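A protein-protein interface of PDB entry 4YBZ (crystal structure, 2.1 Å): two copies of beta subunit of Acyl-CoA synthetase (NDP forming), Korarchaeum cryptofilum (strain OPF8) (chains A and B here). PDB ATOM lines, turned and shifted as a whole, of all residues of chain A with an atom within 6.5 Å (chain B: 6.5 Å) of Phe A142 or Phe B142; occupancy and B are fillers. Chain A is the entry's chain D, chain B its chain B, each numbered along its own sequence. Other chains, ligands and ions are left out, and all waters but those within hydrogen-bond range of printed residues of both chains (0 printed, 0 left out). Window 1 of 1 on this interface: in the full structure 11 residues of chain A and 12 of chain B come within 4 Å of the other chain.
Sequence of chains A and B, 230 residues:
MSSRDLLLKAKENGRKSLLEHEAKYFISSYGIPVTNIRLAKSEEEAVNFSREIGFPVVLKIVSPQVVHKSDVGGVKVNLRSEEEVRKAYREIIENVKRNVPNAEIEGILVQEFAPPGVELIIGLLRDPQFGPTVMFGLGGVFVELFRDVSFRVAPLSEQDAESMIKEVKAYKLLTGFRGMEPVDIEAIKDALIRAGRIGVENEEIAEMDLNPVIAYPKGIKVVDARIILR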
ATOM      1  N   ILE A 121      -8.739 -18.923   3.513  1.00  0.00           N
ATOM      2  CA  ILE A 121      -8.167 -19.144   2.195  1.00  0.00           C
ATOM      3  C   ILE A 121      -8.521 -17.954   1.314  1.00  0.00           C
ATOM      4  O   ILE A 121      -9.692 -17.578   1.208  1.00  0.00           O
ATOM      5  CB  ILE A 121      -8.686 -20.446   1.561  1.00  0.00           C
ATOM      6  CG1 ILE A 121      -8.419 -21.636   2.489  1.00  0.00           C
ATOM      7  CG2 ILE A 121      -8.026 -20.676   0.204  1.00  0.00           C
ATOM      8  CD1 ILE A 121      -9.384 -22.771   2.305  1.00  0.00           C
ATOM      9  N   GLY A 137     -12.716 -17.846   1.521  1.00  0.00           N
ATOM     10  CA  GLY A 137     -13.409 -18.848   2.305  1.00  0.00           C
ATOM     11  C   GLY A 137     -12.700 -19.165   3.606  1.00  0.00           C
ATOM     12  O   GLY A 137     -11.540 -18.799   3.795  1.00  0.00           O
ATOM     13  N   LEU A 138     -13.402 -19.847   4.505  1.00  0.00           N
ATOM     14  CA  LEU A 138     -12.811 -20.308   5.757  1.00  0.00           C
ATOM     15  C   LEU A 138     -12.000 -21.572   5.512  1.00  0.00           C
ATOM     16  O   LEU A 138     -12.346 -22.397   4.667  1.00  0.00           O
ATOM     17  CB  LEU A 138     -13.893 -20.561   6.810  1.00  0.00           C
ATOM     18  CG  LEU A 138     -14.298 -19.357   7.666  1.00  0.00           C
ATOM     19  CD1 LEU A 138     -13.188 -19.021   8.650  1.00  0.00           C
ATOM     20  CD2 LEU A 138     -14.628 -18.145   6.806  1.00  0.00           C
ATOM     21  N   GLY A 139     -10.909 -21.715   6.253  1.00  0.00           N
ATOM     22  CA  GLY A 139      -9.991 -22.814   6.033  1.00  0.00           C
ATOM     23  C   GLY A 139     -10.549 -24.146   6.490  1.00  0.00           C
ATOM     24  O   GLY A 139     -11.714 -24.248   6.886  1.00  0.00           O
ATOM     25  N   GLY A 140      -9.697 -25.163   6.451  1.00  0.00           N
ATOM     26  CA  GLY A 140     -10.080 -26.501   6.853  1.00  0.00           C
ATOM     27  C   GLY A 140     -11.205 -27.079   6.018  1.00  0.00           C
ATOM     28  O   GLY A 140     -11.249 -26.915   4.795  1.00  0.00           O
ATOM     29  N   VAL A 141     -12.119 -27.758   6.699  1.00  0.00           N
ATOM     30  CA  VAL A 141     -13.205 -28.474   6.046  1.00  0.00           C
ATOM     31  C   VAL A 141     -14.215 -27.537   5.391  1.00  0.00           C
ATOM     32  O   VAL A 141     -15.112 -27.990   4.683  1.00  0.00           O
ATOM     33  CB  VAL A 141     -13.959 -29.375   7.048  1.00  0.00           C
ATOM     34  CG1 VAL A 141     -13.035 -30.462   7.581  1.00  0.00           C
ATOM     35  CG2 VAL A 141     -14.527 -28.547   8.198  1.00  0.00           C
ATOM     36  N   PHE A 142     -14.113 -26.243   5.671  1.00  0.00           N
ATOM     37  CA  PHE A 142     -15.125 -25.301   5.204  1.00  0.00           C
ATOM     38  C   PHE A 142     -15.010 -25.014   3.710  1.00  0.00           C
ATOM     39  O   PHE A 142     -16.026 -24.886   3.029  1.00  0.00           O
ATOM     40  CB  PHE A 142     -15.048 -24.018   6.026  1.00  0.00           C
ATOM     41  CG  PHE A 142     -15.440 -24.218   7.460  1.00  0.00           C
ATOM     42  CD1 PHE A 142     -16.775 -24.318   7.813  1.00  0.00           C
ATOM     43  CD2 PHE A 142     -14.479 -24.349   8.447  1.00  0.00           C
ATOM     44  CE1 PHE A 142     -17.145 -24.520   9.125  1.00  0.00           C
ATOM     45  CE2 PHE A 142     -14.844 -24.552   9.762  1.00  0.00           C
ATOM     46  CZ  PHE A 142     -16.177 -24.640  10.101  1.00  0.00           C
ATOM     47  N   VAL A 143     -13.788 -24.907   3.201  1.00  0.00           N
ATOM     48  CA  VAL A 143     -13.582 -24.853   1.755  1.00  0.00           C
ATOM     49  C   VAL A 143     -13.315 -26.253   1.222  1.00  0.00           C
ATOM     50  O   VAL A 143     -13.922 -26.682   0.237  1.00  0.00           O
ATOM     51  CB  VAL A 143     -12.419 -23.920   1.362  1.00  0.00           C
ATOM     52  CG1 VAL A 143     -12.000 -24.144  -0.096  1.00  0.00           C
ATOM     53  CG2 VAL A 143     -12.824 -22.478   1.561  1.00  0.00           C
ATOM     54  N   GLU A 144     -12.414 -26.965   1.892  1.00  0.00           N
ATOM     55  CA  GLU A 144     -11.922 -28.244   1.394  1.00  0.00           C
ATOM     56  C   GLU A 144     -13.020 -29.302   1.268  1.00  0.00           C
ATOM     57  O   GLU A 144     -13.025 -30.077   0.312  1.00  0.00           O
ATOM     58  CB  GLU A 144     -10.808 -28.758   2.307  1.00  0.00           C
ATOM     59  CG  GLU A 144     -10.076 -29.984   1.779  1.00  0.00           C
ATOM     60  CD  GLU A 144      -8.769 -30.248   2.504  1.00  0.00           C
ATOM     61  OE1 GLU A 144      -8.392 -29.443   3.383  1.00  0.00           O
ATOM     62  OE2 GLU A 144      -8.113 -31.261   2.183  1.00  0.00           O
ATOM     63  N   LEU A 145     -13.947 -29.327   2.223  1.00  0.00           N
ATOM     64  CA  LEU A 145     -15.000 -30.344   2.246  1.00  0.00           C
ATOM     65  C   LEU A 145     -16.364 -29.797   1.820  1.00  0.00           C
ATOM     66  O   LEU A 145     -17.050 -30.409   1.002  1.00  0.00           O
ATOM     67  CB  LEU A 145     -15.096 -30.968   3.641  1.00  0.00           C
ATOM     68  CG  LEU A 145     -15.960 -32.222   3.779  1.00  0.00           C
ATOM     69  CD1 LEU A 145     -15.384 -33.378   2.975  1.00  0.00           C
ATOM     70  CD2 LEU A 145     -16.082 -32.604   5.247  1.00  0.00           C
ATOM     71  N   PHE A 146     -16.752 -28.647   2.367  1.00  0.00           N
ATOM     72  CA  PHE A 146     -18.090 -28.096   2.138  1.00  0.00           C
ATOM     73  C   PHE A 146     -18.155 -27.171   0.921  1.00  0.00           C
ATOM     74  O   PHE A 146     -19.243 -26.843   0.446  1.00  0.00           O
ATOM     75  CB  PHE A 146     -18.573 -27.341   3.380  1.00  0.00           C
ATOM     76  CG  PHE A 146     -18.713 -28.205   4.603  1.00  0.00           C
ATOM     77  CD1 PHE A 146     -19.275 -29.470   4.519  1.00  0.00           C
ATOM     78  CD2 PHE A 146     -18.276 -27.756   5.837  1.00  0.00           C
ATOM     79  CE1 PHE A 146     -19.404 -30.261   5.644  1.00  0.00           C
ATOM     80  CE2 PHE A 146     -18.403 -28.547   6.964  1.00  0.00           C
ATOM     81  CZ  PHE A 146     -18.966 -29.800   6.864  1.00  0.00           C
ATOM     82  N   ARG A 147     -16.992 -26.784   0.401  1.00  0.00           N
ATOM     83  CA  ARG A 147     -16.909 -25.905  -0.766  1.00  0.00           C
ATOM     84  C   ARG A 147     -17.593 -24.560  -0.514  1.00  0.00           C
ATOM     85  O   ARG A 147     -18.171 -23.961  -1.418  1.00  0.00           O
ATOM     86  CB  ARG A 147     -17.553 -26.582  -1.985  1.00  0.00           C
ATOM     87  CG  ARG A 147     -16.949 -27.927  -2.356  1.00  0.00           C
ATOM     88  CD  ARG A 147     -15.606 -27.773  -3.037  1.00  0.00           C
ATOM     89  NE  ARG A 147     -14.745 -28.935  -2.824  1.00  0.00           N
ATOM     90  CZ  ARG A 147     -14.803 -30.060  -3.531  1.00  0.00           C
ATOM     91  NH1 ARG A 147     -15.689 -30.201  -4.509  1.00  0.00           N
ATOM     92  NH2 ARG A 147     -13.970 -31.054  -3.253  1.00  0.00           N
ATOM     93  N   ASP A 148     -17.460 -24.038   0.699  1.00  0.00           N
ATOM     94  CA  ASP A 148     -18.105 -22.776   1.049  1.00  0.00           C
ATOM     95  C   ASP A 148     -17.215 -21.576   0.733  1.00  0.00           C
ATOM     96  O   ASP A 148     -16.393 -21.186   1.559  1.00  0.00           O
ATOM     97  CB  ASP A 148     -18.476 -22.771   2.534  1.00  0.00           C
ATOM     98  CG  ASP A 148     -19.064 -21.450   2.988  1.00  0.00           C
ATOM     99  OD1 ASP A 148     -19.720 -20.775   2.168  1.00  0.00           O
ATOM    100  OD2 ASP A 148     -18.875 -21.094   4.170  1.00  0.00           O
ATOM    101  N   VAL A 149     -17.423 -20.967  -0.434  1.00  0.00           N
ATOM    102  CA  VAL A 149     -16.545 -19.901  -0.919  1.00  0.00           C
ATOM    103  C   VAL A 149     -17.332 -18.811  -1.632  1.00  0.00           C
ATOM    104  O   VAL A 149     -18.396 -19.070  -2.195  1.00  0.00           O
ATOM    105  CB  VAL A 149     -15.465 -20.420  -1.898  1.00  0.00           C
ATOM    106  CG1 VAL A 149     -14.527 -21.378  -1.206  1.00  0.00           C
ATOM    107  CG2 VAL A 149     -16.102 -21.071  -3.121  1.00  0.00           C
ATOM    108  N   ALA A 170     -19.821 -19.707   6.610  1.00  0.00           N
ATOM    109  CA  ALA A 170     -19.010 -19.860   7.818  1.00  0.00           C
ATOM    110  C   ALA A 170     -18.503 -18.516   8.337  1.00  0.00           C
ATOM    111  O   ALA A 170     -17.517 -18.458   9.078  1.00  0.00           O
ATOM    112  CB  ALA A 170     -17.841 -20.793   7.541  1.00  0.00           C
ATOM    113  N   LEU A 173     -17.633 -17.521  12.030  1.00  0.00           N
ATOM    114  CA  LEU A 173     -16.351 -17.912  12.622  1.00  0.00           C
ATOM    115  C   LEU A 173     -15.399 -16.725  12.775  1.00  0.00           C
ATOM    116  O   LEU A 173     -14.386 -16.831  13.464  1.00  0.00           O
ATOM    117  CB  LEU A 173     -15.652 -18.988  11.787  1.00  0.00           C
ATOM    118  CG  LEU A 173     -16.231 -20.400  11.706  1.00  0.00           C
ATOM    119  CD1 LEU A 173     -15.232 -21.291  10.983  1.00  0.00           C
ATOM    120  CD2 LEU A 173     -16.575 -20.972  13.072  1.00  0.00           C
ATOM    121  N   ILE B 121     -24.001 -34.210  18.655  1.00  0.00           N
ATOM    122  CA  ILE B 121     -25.009 -33.919  19.664  1.00  0.00           C
ATOM    123  C   ILE B 121     -26.300 -34.649  19.333  1.00  0.00           C
ATOM    124  O   ILE B 121     -26.806 -34.571  18.212  1.00  0.00           O
ATOM    125  CB  ILE B 121     -25.290 -32.416  19.790  1.00  0.00           C
ATOM    126  CG1 ILE B 121     -24.009 -31.670  20.168  1.00  0.00           C
ATOM    127  CG2 ILE B 121     -26.347 -32.162  20.866  1.00  0.00           C
ATOM    128  CD1 ILE B 121     -24.002 -30.229  19.743  1.00  0.00           C
ATOM    129  N   GLY B 137     -27.192 -33.261  15.477  1.00  0.00           N
ATOM    130  CA  GLY B 137     -26.294 -32.316  14.838  1.00  0.00           C
ATOM    131  C   GLY B 137     -24.835 -32.613  15.124  1.00  0.00           C
ATOM    132  O   GLY B 137     -24.514 -33.398  16.016  1.00  0.00           O
ATOM    133  N   LEU B 138     -23.948 -31.981  14.361  1.00  0.00           N
ATOM    134  CA  LEU B 138     -22.513 -32.107  14.592  1.00  0.00           C
ATOM    135  C   LEU B 138     -22.091 -31.201  15.747  1.00  0.00           C
ATOM    136  O   LEU B 138     -22.656 -30.126  15.947  1.00  0.00           O
ATOM    137  CB  LEU B 138     -21.728 -31.766  13.324  1.00  0.00           C
ATOM    138  CG  LEU B 138     -21.514 -32.912  12.331  1.00  0.00           C
ATOM    139  CD1 LEU B 138     -20.525 -33.931  12.884  1.00  0.00           C
ATOM    140  CD2 LEU B 138     -22.832 -33.585  11.967  1.00  0.00           C
ATOM    141  N   GLY B 139     -21.103 -31.641  16.518  1.00  0.00           N
ATOM    142  CA  GLY B 139     -20.711 -30.918  17.713  1.00  0.00           C
ATOM    143  C   GLY B 139     -19.984 -29.623  17.412  1.00  0.00           C
ATOM    144  O   GLY B 139     -19.843 -29.223  16.251  1.00  0.00           O
ATOM    145  N   GLY B 140     -19.496 -28.984  18.471  1.00  0.00           N
ATOM    146  CA  GLY B 140     -18.789 -27.726  18.350  1.00  0.00           C
ATOM    147  C   GLY B 140     -19.636 -26.622  17.743  1.00  0.00           C
ATOM    148  O   GLY B 140     -20.824 -26.482  18.050  1.00  0.00           O
ATOM    149  N   VAL B 141     -19.008 -25.841  16.872  1.00  0.00           N
ATOM    150  CA  VAL B 141     -19.639 -24.672  16.273  1.00  0.00           C
ATOM    151  C   VAL B 141     -20.772 -25.005  15.312  1.00  0.00           C
ATOM    152  O   VAL B 141     -21.490 -24.108  14.870  1.00  0.00           O
ATOM    153  CB  VAL B 141     -18.609 -23.820  15.499  1.00  0.00           C
ATOM    154  CG1 VAL B 141     -17.604 -23.190  16.451  1.00  0.00           C
ATOM    155  CG2 VAL B 141     -17.909 -24.657  14.424  1.00  0.00           C
ATOM    156  N   PHE B 142     -20.912 -26.273  14.945  1.00  0.00           N
ATOM    157  CA  PHE B 142     -21.886 -26.626  13.918  1.00  0.00           C
ATOM    158  C   PHE B 142     -23.307 -26.558  14.463  1.00  0.00           C
ATOM    159  O   PHE B 142     -24.216 -26.126  13.757  1.00  0.00           O
ATOM    160  CB  PHE B 142     -21.578 -28.002  13.339  1.00  0.00           C
ATOM    161  CG  PHE B 142     -20.290 -28.044  12.569  1.00  0.00           C
ATOM    162  CD1 PHE B 142     -20.222 -27.522  11.287  1.00  0.00           C
ATOM    163  CD2 PHE B 142     -19.147 -28.580  13.130  1.00  0.00           C
ATOM    164  CE1 PHE B 142     -19.039 -27.545  10.577  1.00  0.00           C
ATOM    165  CE2 PHE B 142     -17.961 -28.607  12.424  1.00  0.00           C
ATOM    166  CZ  PHE B 142     -17.907 -28.087  11.147  1.00  0.00           C
ATOM    167  N   VAL B 143     -23.496 -26.972  15.710  1.00  0.00           N
ATOM    168  CA  VAL B 143     -24.780 -26.762  16.377  1.00  0.00           C
ATOM    169  C   VAL B 143     -24.780 -25.458  17.173  1.00  0.00           C
ATOM    170  O   VAL B 143     -25.699 -24.648  17.025  1.00  0.00           O
ATOM    171  CB  VAL B 143     -25.139 -27.946  17.298  1.00  0.00           C
ATOM    172  CG1 VAL B 143     -26.264 -27.578  18.268  1.00  0.00           C
ATOM    173  CG2 VAL B 143     -25.553 -29.144  16.461  1.00  0.00           C
ATOM    174  N   GLU B 144     -23.757 -25.235  17.996  1.00  0.00           N
ATOM    175  CA  GLU B 144     -23.770 -24.084  18.900  1.00  0.00           C
ATOM    176  C   GLU B 144     -23.784 -22.744  18.169  1.00  0.00           C
ATOM    177  O   GLU B 144     -24.434 -21.801  18.620  1.00  0.00           O
ATOM    178  CB  GLU B 144     -22.581 -24.112  19.861  1.00  0.00           C
ATOM    179  CG  GLU B 144     -22.661 -22.999  20.910  1.00  0.00           C
ATOM    180  CD  GLU B 144     -21.735 -23.204  22.089  1.00  0.00           C
ATOM    181  OE1 GLU B 144     -21.067 -24.254  22.149  1.00  0.00           O
ATOM    182  OE2 GLU B 144     -21.675 -22.306  22.957  1.00  0.00           O
ATOM    183  N   LEU B 145     -23.073 -22.658  17.049  1.00  0.00           N
ATOM    184  CA  LEU B 145     -22.958 -21.395  16.324  1.00  0.00           C
ATOM    185  C   LEU B 145     -23.844 -21.353  15.085  1.00  0.00           C
ATOM    186  O   LEU B 145     -24.562 -20.379  14.867  1.00  0.00           O
ATOM    187  CB  LEU B 145     -21.505 -21.145  15.914  1.00  0.00           C
ATOM    188  CG  LEU B 145     -21.191 -19.748  15.380  1.00  0.00           C
ATOM    189  CD1 LEU B 145     -21.357 -18.690  16.463  1.00  0.00           C
ATOM    190  CD2 LEU B 145     -19.790 -19.713  14.787  1.00  0.00           C
ATOM    191  N   PHE B 146     -23.799 -22.406  14.275  1.00  0.00           N
ATOM    192  CA  PHE B 146     -24.510 -22.402  13.000  1.00  0.00           C
ATOM    193  C   PHE B 146     -25.922 -22.970  13.107  1.00  0.00           C
ATOM    194  O   PHE B 146     -26.722 -22.809  12.184  1.00  0.00           O
ATOM    195  CB  PHE B 146     -23.714 -23.185  11.951  1.00  0.00           C
ATOM    196  CG  PHE B 146     -22.356 -22.606  11.663  1.00  0.00           C
ATOM    197  CD1 PHE B 146     -22.179 -21.238  11.550  1.00  0.00           C
ATOM    198  CD2 PHE B 146     -21.257 -23.432  11.500  1.00  0.00           C
ATOM    199  CE1 PHE B 146     -20.934 -20.707  11.285  1.00  0.00           C
ATOM    200  CE2 PHE B 146     -20.008 -22.902  11.234  1.00  0.00           C
ATOM    201  CZ  PHE B 146     -19.849 -21.539  11.126  1.00  0.00           C
ATOM    202  N   ARG B 147     -26.227 -23.630  14.222  1.00  0.00           N
ATOM    203  CA  ARG B 147     -27.552 -24.210  14.427  1.00  0.00           C
ATOM    204  C   ARG B 147     -27.916 -25.175  13.304  1.00  0.00           C
ATOM    205  O   ARG B 147     -29.047 -25.184  12.819  1.00  0.00           O
ATOM    206  CB  ARG B 147     -28.619 -23.116  14.555  1.00  0.00           C
ATOM    207  CG  ARG B 147     -28.402 -22.183  15.745  1.00  0.00           C
ATOM    208  CD  ARG B 147     -28.699 -22.839  17.108  1.00  0.00           C
ATOM    209  NE  ARG B 147     -29.603 -23.992  17.045  1.00  0.00           N
ATOM    210  CZ  ARG B 147     -30.215 -24.525  18.097  1.00  0.00           C
ATOM    211  NH1 ARG B 147     -31.013 -25.575  17.935  1.00  0.00           N
ATOM    212  NH2 ARG B 147     -30.047 -24.016  19.313  1.00  0.00           N
ATOM    213  N   ASP B 148     -26.942 -25.981  12.897  1.00  0.00           N
ATOM    214  CA  ASP B 148     -27.144 -26.965  11.845  1.00  0.00           C
ATOM    215  C   ASP B 148     -27.678 -28.209  12.531  1.00  0.00           C
ATOM    216  O   ASP B 148     -26.927 -28.972  13.143  1.00  0.00           O
ATOM    217  CB  ASP B 148     -25.851 -27.258  11.092  1.00  0.00           C
ATOM    218  CG  ASP B 148     -26.018 -28.345  10.056  1.00  0.00           C
ATOM    219  OD1 ASP B 148     -27.129 -28.464   9.497  1.00  0.00           O
ATOM    220  OD2 ASP B 148     -25.043 -29.078   9.800  1.00  0.00           O
ATOM    221  N   VAL B 149     -28.995 -28.367  12.489  1.00  0.00           N
ATOM    222  CA  VAL B 149     -29.661 -29.388  13.283  1.00  0.00           C
ATOM    223  C   VAL B 149     -30.855 -29.993  12.546  1.00  0.00           C
ATOM    224  O   VAL B 149     -31.507 -29.322  11.747  1.00  0.00           O
ATOM    225  CB  VAL B 149     -30.097 -28.772  14.641  1.00  0.00           C
ATOM    226  CG1 VAL B 149     -31.615 -28.615  14.744  1.00  0.00           C
ATOM    227  CG2 VAL B 149     -29.552 -29.585  15.796  1.00  0.00           C
ATOM    228  N   LYS B 169     -26.269 -30.091   7.373  1.00  0.00           N
ATOM    229  CA  LYS B 169     -25.310 -29.497   6.442  1.00  0.00           C
ATOM    230  C   LYS B 169     -23.892 -30.025   6.664  1.00  0.00           C
ATOM    231  O   LYS B 169     -23.068 -29.995   5.752  1.00  0.00           O
ATOM    232  CB  LYS B 169     -25.334 -27.967   6.554  1.00  0.00           C
ATOM    233  CG  LYS B 169     -26.586 -27.331   5.955  1.00  0.00           C
ATOM    234  CD  LYS B 169     -26.873 -25.942   6.513  1.00  0.00           C
ATOM    235  CE  LYS B 169     -28.369 -25.656   6.544  1.00  0.00           C
ATOM    236  NZ  LYS B 169     -28.693 -24.299   6.023  1.00  0.00           N
ATOM    237  N   ALA B 170     -23.606 -30.469   7.884  1.00  0.00           N
ATOM    238  CA  ALA B 170     -22.275 -30.952   8.250  1.00  0.00           C
ATOM    239  C   ALA B 170     -22.157 -32.476   8.130  1.00  0.00           C
ATOM    240  O   ALA B 170     -21.289 -33.089   8.760  1.00  0.00           O
ATOM    241  CB  ALA B 170     -21.942 -30.513   9.668  1.00  0.00           C
ATOM    242  N   LEU B 173     -18.933 -34.654   7.445  1.00  0.00           N
ATOM    243  CA  LEU B 173     -17.970 -34.863   8.524  1.00  0.00           C
ATOM    244  C   LEU B 173     -18.007 -36.290   9.058  1.00  0.00           C
ATOM    245  O   LEU B 173     -17.106 -36.709   9.785  1.00  0.00           O
ATOM    246  CB  LEU B 173     -18.231 -33.882   9.670  1.00  0.00           C
ATOM    247  CG  LEU B 173     -17.944 -32.400   9.425  1.00  0.00           C
ATOM    248  CD1 LEU B 173     -18.135 -31.628  10.715  1.00  0.00           C
ATOM    249  CD2 LEU B 173     -16.536 -32.179   8.889  1.00  0.00           C
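The backbone carbonyl oxygen of Val B141 is in hydrogen-bond range of the backbone NH of Phe B146.
The backbone NH (N) of Arg B147 lies within hydrogen-bond range of the backbone carbonyl oxygen (O) of Phe B142.
OD1 of Asp B148 is in hydrogen-bond range of N of Lys B169, 2.8 Å away.
The backbone carbonyl oxygen (O) of Phe A142 lies within hydrogen-bond range of the backbone NH (N) of Arg A147 (3.4 Å).
N of Asp A148 lies within hydrogen-bond range of O of Phe A142, 2.9 Å away.
OD2 of Asp A148 sits at hydrogen-bond distance from N of Ala A170.
Among the printed residues, merely in contact across the chains: Phe A146 with Lys B169 (3.7 Å), Leu A145 with Leu B173 (3.7 Å), Phe A146 with Ala B170 (3.8 Å), Phe A146 with Leu B173 (3.8 Å), Phe A146 with Phe B142 (3.8 Å), Ala A170 with Phe B146 (3.8 Å), Leu A173 with Phe B146 (3.8 Å), Phe A142 with Phe B142 (3.9 Å), Leu A173 with Leu B145 (3.9 Å) and Phe A142 with Phe B146 (3.9 Å).
Of chain B, only Phe B142 and Phe B146 come within 4 Å of Phe A142.
Phe B142 touches just these residues of chain A: Phe A142 (3.9 Å) and Phe A146 (3.8 Å).
Printed residues of chain B within 4 Å of Ala A170: Phe B146.
Printed residues of chain A within 4 Å of Leu B173: Leu A145 and Phe A146.
Printed residues of chain A within 4 Å of Leu B145: Leu A173.
Printed residues of chain B within 4 Å of Leu A145: Leu B173 (3.7 Å).
Gly A137 touches none of the printed residues of chain B.
Ile A121 touches none of the printed residues of chain B.
The nearest residue of chain B that does not touch Phe A142 is Val B141 (4.7 Å).
The nearest residue of chain A that does not touch Phe B142 is Val A141 (4.5 Å).
Printed residues of chain B that touch a printed residue of chain A: Phe B142, Leu B145, Phe B146, Lys B169, Ala B170 and Leu B173.
Hydrophobic or aromatic side chains of chain B that line the printed part of chain A: Phe B142, Leu B145, Phe B146 and Leu B173.
Along chain A the printed residues that touch a printed residue of chain B span positions 142 to 173.
Among the printed residues, 10 pairs touch across the chains.
Among the printed residues, no Asp or Glu carboxylate lies within 4 Å of a Lys or Arg side-chain nitrogen of the other chain.
Phe B142 touches its own counterpart, Phe A142.
Phe A142 touches Phe B146, and with the chains exchanged Phe A146 touches Phe B142.
Leu A145 touches Leu B173, and with the chains exchanged Leu A173 touches Leu B145.
Phe A146 touches Ala B170, and with the chains exchanged Ala A170 touches Phe B146.
Positions printed for both chains: 121, 137, 138, 139, 140, 141, 142, 143, 144, 145, 146, 147, 148, 149, 170 and 173.
Of the 10 pairs that touch across the chains among the printed residues, 9 have their exchanged pair printed and touching as well.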
